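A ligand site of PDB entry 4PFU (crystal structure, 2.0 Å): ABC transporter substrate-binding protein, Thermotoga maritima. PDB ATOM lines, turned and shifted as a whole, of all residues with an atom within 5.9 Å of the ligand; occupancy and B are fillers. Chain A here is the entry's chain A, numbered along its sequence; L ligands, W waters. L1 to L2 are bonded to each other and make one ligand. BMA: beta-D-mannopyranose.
NE1 of Trp 371 sits close to OH of Tyr 293, at 3.4 Å. The side-chain hydroxyl (OH) of Tyr 293 is in hydrogen-bond range of the side-chain carboxylate (OD2) of Asp 370, at 2.5 Å. OG1 of Thr 369 sits at hydrogen-bond distance from ND2 of Asn 212 (3.0 Å). The side-chain amide nitrogen (ND2) of Asn 228 is in hydrogen-bond range of the backbone carbonyl oxygen (O) of Ala 498. NE1 of Trp 16 lies within hydrogen-bond range of O of Gly 13. N of Asn 212 is in hydrogen-bond range of O of Gly 367 (3.1 Å).
Water W7 lies within hydrogen-bond range of an oxygen (O6) of BMA L2 and the indole nitrogen (NE1) of Trp 371. Water W5 lies within hydrogen-bond range of OH of Tyr 400 (2.7 Å) and O6 of BMA L1 (2.8 Å). Water W6 bridges the side-chain hydroxyl (OG1) of Thr 257 (2.8 Å) and an oxygen (O3) of BMA L1 (2.8 Å). Water W2 lies within hydrogen-bond range of the side-chain hydroxyl (OH) of Tyr 400, the side-chain amide nitrogen (ND2) of Asn 415 and an oxygen (O1) of BMA L1. Water W3 lies within hydrogen-bond range of the indole nitrogen of Trp 522 (2.9 Å), an oxygen (O2) of BMA L2 (2.9 Å) and the backbone carbonyl oxygen of Asn 228 (3.0 Å). Water W1 lies within hydrogen-bond range of O of Ala 414 (2.8 Å), O1 of BMA L1 (3.2 Å) and N of Gly 416 (3.4 Å).
Residues that only touch the ligand: Phe 229, Trp 368, Gly 13, Ser 14, Trp 522, Asn 415 and Ala 414. Hydrophobic or aromatic side chains within 4 Å of the ligand: Trp 16, Phe 229, Met 230, Trp 368, Trp 371 and Trp 522. 13 residues have an atom within 4 Å of the ligand: Gly 13, Ser 14, Trp 16, Asn 212, Asn 228, Phe 229, Met 230, Trp 368, Asp 370, Trp 371, Ala 414, Asn 415 and Trp 522.
An oxygen (O2) of BMA L2 lies within hydrogen-bond range of the backbone carbonyl oxygen (O) of Asn 228 (2.8 Å). OD1 of Asn 212 is in hydrogen-bond range of O3 of BMA L2 (2.7 Å). O4 of BMA L2 is in hydrogen-bond range of OD1 of Asp 370 (2.6 Å). The indole nitrogen (NE1) of Trp 16 is in hydrogen-bond range of an oxygen (O6) of BMA L1 (3.4 Å). O3 of BMA L2 is in hydrogen-bond range of N of Met 230. NE1 of Trp 371 lies close to O6 of BMA L2 (3.4 Å).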
ATOM      1  N   GLY A  13      -7.287 -25.162   6.046  1.00  0.00           N
ATOM      2  CA  GLY A  13      -7.313 -25.500   4.629  1.00  0.00           C
ATOM      3  C   GLY A  13      -7.186 -26.975   4.347  1.00  0.00           C
ATOM      4  O   GLY A  13      -7.541 -27.423   3.258  1.00  0.00           O
ATOM      5  N   SER A  14      -6.693 -27.739   5.319  1.00  0.00           N
ATOM      6  CA  SER A  14      -6.375 -29.163   5.088  1.00  0.00           C
ATOM      7  C   SER A  14      -7.087 -30.150   6.004  1.00  0.00           C
ATOM      8  O   SER A  14      -6.830 -31.356   5.941  1.00  0.00           O
ATOM      9  CB  SER A  14      -4.866 -29.372   5.225  1.00  0.00           C
ATOM     10  OG  SER A  14      -4.415 -29.075   6.537  1.00  0.00           O
ATOM     11  N   LEU A  15      -7.958 -29.642   6.868  1.00  0.00           N
ATOM     12  CA  LEU A  15      -8.624 -30.491   7.863  1.00  0.00           C
ATOM     13  C   LEU A  15     -10.102 -30.592   7.545  1.00  0.00           C
ATOM     14  O   LEU A  15     -10.870 -29.684   7.849  1.00  0.00           O
ATOM     15  CB  LEU A  15      -8.418 -29.930   9.277  1.00  0.00           C
ATOM     16  CG  LEU A  15      -9.082 -30.719  10.427  1.00  0.00           C
ATOM     17  CD1 LEU A  15      -8.480 -32.125  10.530  1.00  0.00           C
ATOM     18  CD2 LEU A  15      -8.944 -29.981  11.752  1.00  0.00           C
ATOM     19  N   TRP A  16     -10.511 -31.688   6.918  1.00  0.00           N
ATOM     20  CA  TRP A  16     -11.891 -31.794   6.436  1.00  0.00           C
ATOM     21  C   TRP A  16     -12.679 -32.935   7.072  1.00  0.00           C
ATOM     22  O   TRP A  16     -13.802 -33.229   6.652  1.00  0.00           O
ATOM     23  CB  TRP A  16     -11.884 -31.920   4.913  1.00  0.00           C
ATOM     24  CG  TRP A  16     -11.300 -30.712   4.245  1.00  0.00           C
ATOM     25  CD1 TRP A  16      -9.987 -30.546   3.855  1.00  0.00           C
ATOM     26  CD2 TRP A  16     -11.971 -29.501   3.927  1.00  0.00           C
ATOM     27  NE1 TRP A  16      -9.824 -29.304   3.297  1.00  0.00           N
ATOM     28  CE2 TRP A  16     -11.025 -28.629   3.335  1.00  0.00           C
ATOM     29  CE3 TRP A  16     -13.291 -29.050   4.084  1.00  0.00           C
ATOM     30  CZ2 TRP A  16     -11.355 -27.356   2.885  1.00  0.00           C
ATOM     31  CZ3 TRP A  16     -13.617 -27.783   3.639  1.00  0.00           C
ATOM     32  CH2 TRP A  16     -12.649 -26.942   3.050  1.00  0.00           C
ATOM     33  N   ASN A 212     -15.332 -23.836   2.033  1.00  0.00           N
ATOM     34  CA  ASN A 212     -14.431 -22.704   1.802  1.00  0.00           C
ATOM     35  C   ASN A 212     -15.037 -21.339   2.165  1.00  0.00           C
ATOM     36  O   ASN A 212     -14.354 -20.478   2.700  1.00  0.00           O
ATOM     37  CB  ASN A 212     -13.977 -22.645   0.345  1.00  0.00           C
ATOM     38  CG  ASN A 212     -13.109 -23.817  -0.043  1.00  0.00           C
ATOM     39  OD1 ASN A 212     -12.451 -24.441   0.806  1.00  0.00           O
ATOM     40  ND2 ASN A 212     -13.103 -24.137  -1.336  1.00  0.00           N
ATOM     41  N   ASN A 228      -5.038 -21.906   3.664  1.00  0.00           N
ATOM     42  CA  ASN A 228      -4.887 -22.626   2.402  1.00  0.00           C
ATOM     43  C   ASN A 228      -6.241 -22.900   1.730  1.00  0.00           C
ATOM     44  O   ASN A 228      -6.315 -23.691   0.781  1.00  0.00           O
ATOM     45  CB  ASN A 228      -4.157 -23.961   2.601  1.00  0.00           C
ATOM     46  CG  ASN A 228      -2.667 -23.815   2.799  1.00  0.00           C
ATOM     47  OD1 ASN A 228      -2.046 -24.600   3.524  1.00  0.00           O
ATOM     48  ND2 ASN A 228      -2.073 -22.804   2.159  1.00  0.00           N
ATOM     49  N   PHE A 229      -7.321 -22.298   2.229  1.00  0.00           N
ATOM     50  CA  PHE A 229      -8.624 -22.460   1.558  1.00  0.00           C
ATOM     51  C   PHE A 229      -8.691 -21.729   0.205  1.00  0.00           C
ATOM     52  O   PHE A 229      -8.261 -20.584   0.111  1.00  0.00           O
ATOM     53  CB  PHE A 229      -9.752 -21.913   2.412  1.00  0.00           C
ATOM     54  CG  PHE A 229      -9.944 -22.619   3.711  1.00  0.00           C
ATOM     55  CD1 PHE A 229     -10.609 -23.841   3.756  1.00  0.00           C
ATOM     56  CD2 PHE A 229      -9.482 -22.056   4.894  1.00  0.00           C
ATOM     57  CE1 PHE A 229     -10.803 -24.486   4.946  1.00  0.00           C
ATOM     58  CE2 PHE A 229      -9.667 -22.700   6.094  1.00  0.00           C
ATOM     59  CZ  PHE A 229     -10.329 -23.917   6.127  1.00  0.00           C
ATOM     60  N   MET A 230      -9.228 -22.392  -0.825  1.00  0.00           N
ATOM     61  CA  MET A 230      -9.536 -21.676  -2.065  1.00  0.00           C
ATOM     62  C   MET A 230     -10.562 -20.619  -1.752  1.00  0.00           C
ATOM     63  O   MET A 230     -11.579 -20.886  -1.096  1.00  0.00           O
ATOM     64  CB  MET A 230     -10.079 -22.606  -3.159  1.00  0.00           C
ATOM     65  CG  MET A 230     -10.497 -21.874  -4.482  1.00  0.00           C
ATOM     66  SD  MET A 230     -12.139 -21.078  -4.468  1.00  0.00           S
ATOM     67  CE  MET A 230     -12.280 -20.334  -6.091  1.00  0.00           C
ATOM     68  N   THR A 257      -0.044 -28.629  -7.497  1.00  0.00           N
ATOM     69  CA  THR A 257      -0.529 -29.965  -7.862  1.00  0.00           C
ATOM     70  C   THR A 257      -1.007 -30.074  -9.311  1.00  0.00           C
ATOM     71  O   THR A 257      -1.315 -29.073  -9.976  1.00  0.00           O
ATOM     72  CB  THR A 257      -1.703 -30.391  -6.963  1.00  0.00           C
ATOM     73  OG1 THR A 257      -2.657 -29.322  -6.908  1.00  0.00           O
ATOM     74  CG2 THR A 257      -1.236 -30.733  -5.557  1.00  0.00           C
ATOM     75  N   TYR A 293     -11.635 -20.026 -11.553  1.00  0.00           N
ATOM     76  CA  TYR A 293     -10.450 -19.536 -10.864  1.00  0.00           C
ATOM     77  C   TYR A 293     -10.035 -18.121 -11.255  1.00  0.00           C
ATOM     78  O   TYR A 293      -9.082 -17.590 -10.686  1.00  0.00           O
ATOM     79  CB  TYR A 293      -9.271 -20.485 -11.106  1.00  0.00           C
ATOM     80  CG  TYR A 293      -9.457 -21.815 -10.431  1.00  0.00           C
ATOM     81  CD1 TYR A 293      -9.334 -21.920  -9.043  1.00  0.00           C
ATOM     82  CD2 TYR A 293      -9.782 -22.949 -11.169  1.00  0.00           C
ATOM     83  CE1 TYR A 293      -9.519 -23.134  -8.410  1.00  0.00           C
ATOM     84  CE2 TYR A 293      -9.964 -24.184 -10.527  1.00  0.00           C
ATOM     85  CZ  TYR A 293      -9.836 -24.256  -9.156  1.00  0.00           C
ATOM     86  OH  TYR A 293     -10.006 -25.461  -8.509  1.00  0.00           O
ATOM     87  N   GLY A 367     -17.988 -28.897  -0.093  1.00  0.00           N
ATOM     88  CA  GLY A 367     -17.316 -27.781   0.552  1.00  0.00           C
ATOM     89  C   GLY A 367     -16.060 -27.329  -0.184  1.00  0.00           C
ATOM     90  O   GLY A 367     -15.528 -26.258   0.114  1.00  0.00           O
ATOM     91  N   TRP A 368     -15.577 -28.124  -1.129  1.00  0.00           N
ATOM     92  CA  TRP A 368     -14.460 -27.669  -1.961  1.00  0.00           C
ATOM     93  C   TRP A 368     -15.072 -26.921  -3.140  1.00  0.00           C
ATOM     94  O   TRP A 368     -15.238 -27.470  -4.237  1.00  0.00           O
ATOM     95  CB  TRP A 368     -13.570 -28.832  -2.418  1.00  0.00           C
ATOM     96  CG  TRP A 368     -12.789 -29.496  -1.313  1.00  0.00           C
ATOM     97  CD1 TRP A 368     -12.988 -29.382   0.040  1.00  0.00           C
ATOM     98  CD2 TRP A 368     -11.680 -30.399  -1.477  1.00  0.00           C
ATOM     99  NE1 TRP A 368     -12.078 -30.158   0.722  1.00  0.00           N
ATOM    100  CE2 TRP A 368     -11.263 -30.786  -0.193  1.00  0.00           C
ATOM    101  CE3 TRP A 368     -11.005 -30.912  -2.593  1.00  0.00           C
ATOM    102  CZ2 TRP A 368     -10.193 -31.655   0.019  1.00  0.00           C
ATOM    103  CZ3 TRP A 368      -9.950 -31.767  -2.386  1.00  0.00           C
ATOM    104  CH2 TRP A 368      -9.547 -32.136  -1.092  1.00  0.00           C
ATOM    105  N   THR A 369     -15.436 -25.678  -2.888  1.00  0.00           N
ATOM    106  CA  THR A 369     -16.346 -24.909  -3.751  1.00  0.00           C
ATOM    107  C   THR A 369     -15.869 -24.806  -5.194  1.00  0.00           C
ATOM    108  O   THR A 369     -16.694 -24.893  -6.122  1.00  0.00           O
ATOM    109  CB  THR A 369     -16.522 -23.500  -3.188  1.00  0.00           C
ATOM    110  OG1 THR A 369     -15.224 -22.897  -3.041  1.00  0.00           O
ATOM    111  CG2 THR A 369     -17.207 -23.590  -1.846  1.00  0.00           C
ATOM    112  N   ASP A 370     -14.563 -24.628  -5.379  1.00  0.00           N
ATOM    113  CA  ASP A 370     -13.993 -24.506  -6.706  1.00  0.00           C
ATOM    114  C   ASP A 370     -14.109 -25.809  -7.503  1.00  0.00           C
ATOM    115  O   ASP A 370     -14.405 -25.797  -8.697  1.00  0.00           O
ATOM    116  CB  ASP A 370     -12.518 -24.056  -6.628  1.00  0.00           C
ATOM    117  CG  ASP A 370     -11.657 -24.959  -5.727  1.00  0.00           C
ATOM    118  OD1 ASP A 370     -12.149 -25.470  -4.692  1.00  0.00           O
ATOM    119  OD2 ASP A 370     -10.469 -25.135  -6.068  1.00  0.00           O
ATOM    120  N   TRP A 371     -13.913 -26.945  -6.839  1.00  0.00           N
ATOM    121  CA  TRP A 371     -14.049 -28.217  -7.544  1.00  0.00           C
ATOM    122  C   TRP A 371     -15.508 -28.579  -7.778  1.00  0.00           C
ATOM    123  O   TRP A 371     -15.821 -29.230  -8.771  1.00  0.00           O
ATOM    124  CB  TRP A 371     -13.367 -29.350  -6.774  1.00  0.00           C
ATOM    125  CG  TRP A 371     -11.861 -29.335  -6.894  1.00  0.00           C
ATOM    126  CD1 TRP A 371     -11.082 -28.298  -7.331  1.00  0.00           C
ATOM    127  CD2 TRP A 371     -10.968 -30.413  -6.587  1.00  0.00           C
ATOM    128  NE1 TRP A 371      -9.752 -28.664  -7.313  1.00  0.00           N
ATOM    129  CE2 TRP A 371      -9.650 -29.956  -6.856  1.00  0.00           C
ATOM    130  CE3 TRP A 371     -11.142 -31.719  -6.118  1.00  0.00           C
ATOM    131  CZ2 TRP A 371      -8.533 -30.758  -6.653  1.00  0.00           C
ATOM    132  CZ3 TRP A 371     -10.020 -32.514  -5.911  1.00  0.00           C
ATOM    133  CH2 TRP A 371      -8.736 -32.032  -6.180  1.00  0.00           C
ATOM    134  N   TYR A 400     -12.576 -39.682   0.185  1.00  0.00           N
ATOM    135  CA  TYR A 400     -11.307 -40.400   0.310  1.00  0.00           C
ATOM    136  C   TYR A 400     -11.477 -41.916   0.451  1.00  0.00           C
ATOM    137  O   TYR A 400     -10.681 -42.703  -0.080  1.00  0.00           O
ATOM    138  CB  TYR A 400     -10.491 -39.847   1.498  1.00  0.00           C
ATOM    139  CG  TYR A 400      -9.821 -38.524   1.190  1.00  0.00           C
ATOM    140  CD1 TYR A 400      -8.723 -38.459   0.336  1.00  0.00           C
ATOM    141  CD2 TYR A 400     -10.284 -37.331   1.755  1.00  0.00           C
ATOM    142  CE1 TYR A 400      -8.102 -37.244   0.044  1.00  0.00           C
ATOM    143  CE2 TYR A 400      -9.670 -36.115   1.470  1.00  0.00           C
ATOM    144  CZ  TYR A 400      -8.584 -36.078   0.610  1.00  0.00           C
ATOM    145  OH  TYR A 400      -7.952 -34.885   0.320  1.00  0.00           O
ATOM    146  N   ALA A 414      -6.333 -34.643  -6.885  1.00  0.00           N
ATOM    147  CA  ALA A 414      -5.010 -34.012  -6.868  1.00  0.00           C
ATOM    148  C   ALA A 414      -4.202 -34.613  -5.718  1.00  0.00           C
ATOM    149  O   ALA A 414      -3.389 -33.940  -5.082  1.00  0.00           O
ATOM    150  CB  ALA A 414      -5.130 -32.488  -6.729  1.00  0.00           C
ATOM    151  N   ASN A 415      -4.433 -35.909  -5.484  1.00  0.00           N
ATOM    152  CA  ASN A 415      -3.865 -36.620  -4.365  1.00  0.00           C
ATOM    153  C   ASN A 415      -2.609 -37.354  -4.800  1.00  0.00           C
ATOM    154  O   ASN A 415      -2.705 -38.395  -5.439  1.00  0.00           O
ATOM    155  CB  ASN A 415      -4.883 -37.618  -3.793  1.00  0.00           C
ATOM    156  CG  ASN A 415      -4.606 -37.975  -2.338  1.00  0.00           C
ATOM    157  OD1 ASN A 415      -4.253 -39.112  -2.017  1.00  0.00           O
ATOM    158  ND2 ASN A 415      -4.771 -37.005  -1.458  1.00  0.00           N
ATOM    159  N   GLY A 416      -1.457 -36.804  -4.469  1.00  0.00           N
ATOM    160  CA  GLY A 416      -0.199 -37.438  -4.820  1.00  0.00           C
ATOM    161  C   GLY A 416       0.437 -36.812  -6.055  1.00  0.00           C
ATOM    162  O   GLY A 416       1.517 -37.193  -6.469  1.00  0.00           O
ATOM    163  N   ALA A 496      -3.897 -24.362  -7.700  1.00  0.00           N
ATOM    164  CA  ALA A 496      -3.282 -23.243  -7.013  1.00  0.00           C
ATOM    165  C   ALA A 496      -2.895 -23.651  -5.605  1.00  0.00           C
ATOM    166  O   ALA A 496      -3.657 -24.333  -4.911  1.00  0.00           O
ATOM    167  CB  ALA A 496      -4.224 -22.044  -6.990  1.00  0.00           C
ATOM    168  N   ALA A 498      -3.209 -22.259  -2.853  1.00  0.00           N
ATOM    169  CA  ALA A 498      -3.954 -21.150  -2.265  1.00  0.00           C
ATOM    170  C   ALA A 498      -3.338 -20.779  -0.907  1.00  0.00           C
ATOM    171  O   ALA A 498      -3.146 -21.641  -0.055  1.00  0.00           O
ATOM    172  CB  ALA A 498      -5.416 -21.514  -2.104  1.00  0.00           C
ATOM    173  N   TRP A 522      -0.907 -28.714   4.349  1.00  0.00           N
ATOM    174  CA  TRP A 522      -1.560 -30.012   4.151  1.00  0.00           C
ATOM    175  C   TRP A 522      -0.860 -31.047   5.009  1.00  0.00           C
ATOM    176  O   TRP A 522       0.326 -30.883   5.318  1.00  0.00           O
ATOM    177  CB  TRP A 522      -1.501 -30.449   2.687  1.00  0.00           C
ATOM    178  CG  TRP A 522      -1.982 -29.455   1.673  1.00  0.00           C
ATOM    179  CD1 TRP A 522      -2.706 -28.319   1.896  1.00  0.00           C
ATOM    180  CD2 TRP A 522      -1.745 -29.501   0.270  1.00  0.00           C
ATOM    181  NE1 TRP A 522      -2.944 -27.665   0.704  1.00  0.00           N
ATOM    182  CE2 TRP A 522      -2.354 -28.378  -0.307  1.00  0.00           C
ATOM    183  CE3 TRP A 522      -1.062 -30.406  -0.559  1.00  0.00           C
ATOM    184  CZ2 TRP A 522      -2.317 -28.116  -1.673  1.00  0.00           C
ATOM    185  CZ3 TRP A 522      -1.025 -30.145  -1.926  1.00  0.00           C
ATOM    186  CH2 TRP A 522      -1.648 -29.007  -2.461  1.00  0.00           C
HETATM  187  C1  BMA L   1      -4.393 -31.995  -1.195  1.00  0.00           C
HETATM  188  C2  BMA L   1      -5.066 -31.408  -2.419  1.00  0.00           C
HETATM  189  C3  BMA L   1      -5.521 -29.985  -2.206  1.00  0.00           C
HETATM  190  C4  BMA L   1      -6.275 -29.826  -0.910  1.00  0.00           C
HETATM  191  C5  BMA L   1      -5.402 -30.344   0.203  1.00  0.00           C
HETATM  192  C6  BMA L   1      -5.946 -30.071   1.586  1.00  0.00           C
HETATM  193  O1  BMA L   1      -4.180 -33.337  -1.320  1.00  0.00           O
HETATM  194  O2  BMA L   1      -6.229 -32.199  -2.689  1.00  0.00           O
HETATM  195  O3  BMA L   1      -6.310 -29.606  -3.343  1.00  0.00           O
HETATM  196  O4  BMA L   1      -6.607 -28.438  -0.595  1.00  0.00           O
HETATM  197  O5  BMA L   1      -5.239 -31.781  -0.002  1.00  0.00           O
HETATM  198  O6  BMA L   1      -7.205 -30.712   1.722  1.00  0.00           O
HETATM  199  C1  BMA L   2      -7.969 -28.175  -0.823  1.00  0.00           C
HETATM  200  C2  BMA L   2      -8.348 -26.877  -0.143  1.00  0.00           C
HETATM  201  C3  BMA L   2      -9.724 -26.444  -0.535  1.00  0.00           C
HETATM  202  C4  BMA L   2      -9.923 -26.421  -2.020  1.00  0.00           C
HETATM  203  C5  BMA L   2      -9.538 -27.776  -2.604  1.00  0.00           C
HETATM  204  C6  BMA L   2      -9.699 -27.786  -4.100  1.00  0.00           C
HETATM  205  O2  BMA L   2      -7.423 -25.841  -0.568  1.00  0.00           O
HETATM  206  O3  BMA L   2      -9.974 -25.117   0.026  1.00  0.00           O
HETATM  207  O4  BMA L   2     -11.303 -26.208  -2.302  1.00  0.00           O
HETATM  208  O5  BMA L   2      -8.147 -28.062  -2.277  1.00  0.00           O
HETATM  209  O6  BMA L   2      -8.901 -26.742  -4.670  1.00  0.00           O
HETATM  210  O   HOH W   1      -1.453 -33.741  -3.029  1.00  0.00           O
HETATM  211  O   HOH W   2      -6.521 -35.001  -1.887  1.00  0.00           O
HETATM  212  O   HOH W   3      -4.495 -25.650  -0.603  1.00  0.00           O
HETATM  213  O   HOH W   4      -6.779 -25.216  -3.308  1.00  0.00           O
HETATM  214  O   HOH W   5      -7.750 -33.320   2.542  1.00  0.00           O
HETATM  215  O   HOH W   6      -5.187 -28.916  -5.816  1.00  0.00           O
HETATM  216  O   HOH W   7      -7.183 -27.256  -6.670  1.00  0.00           O
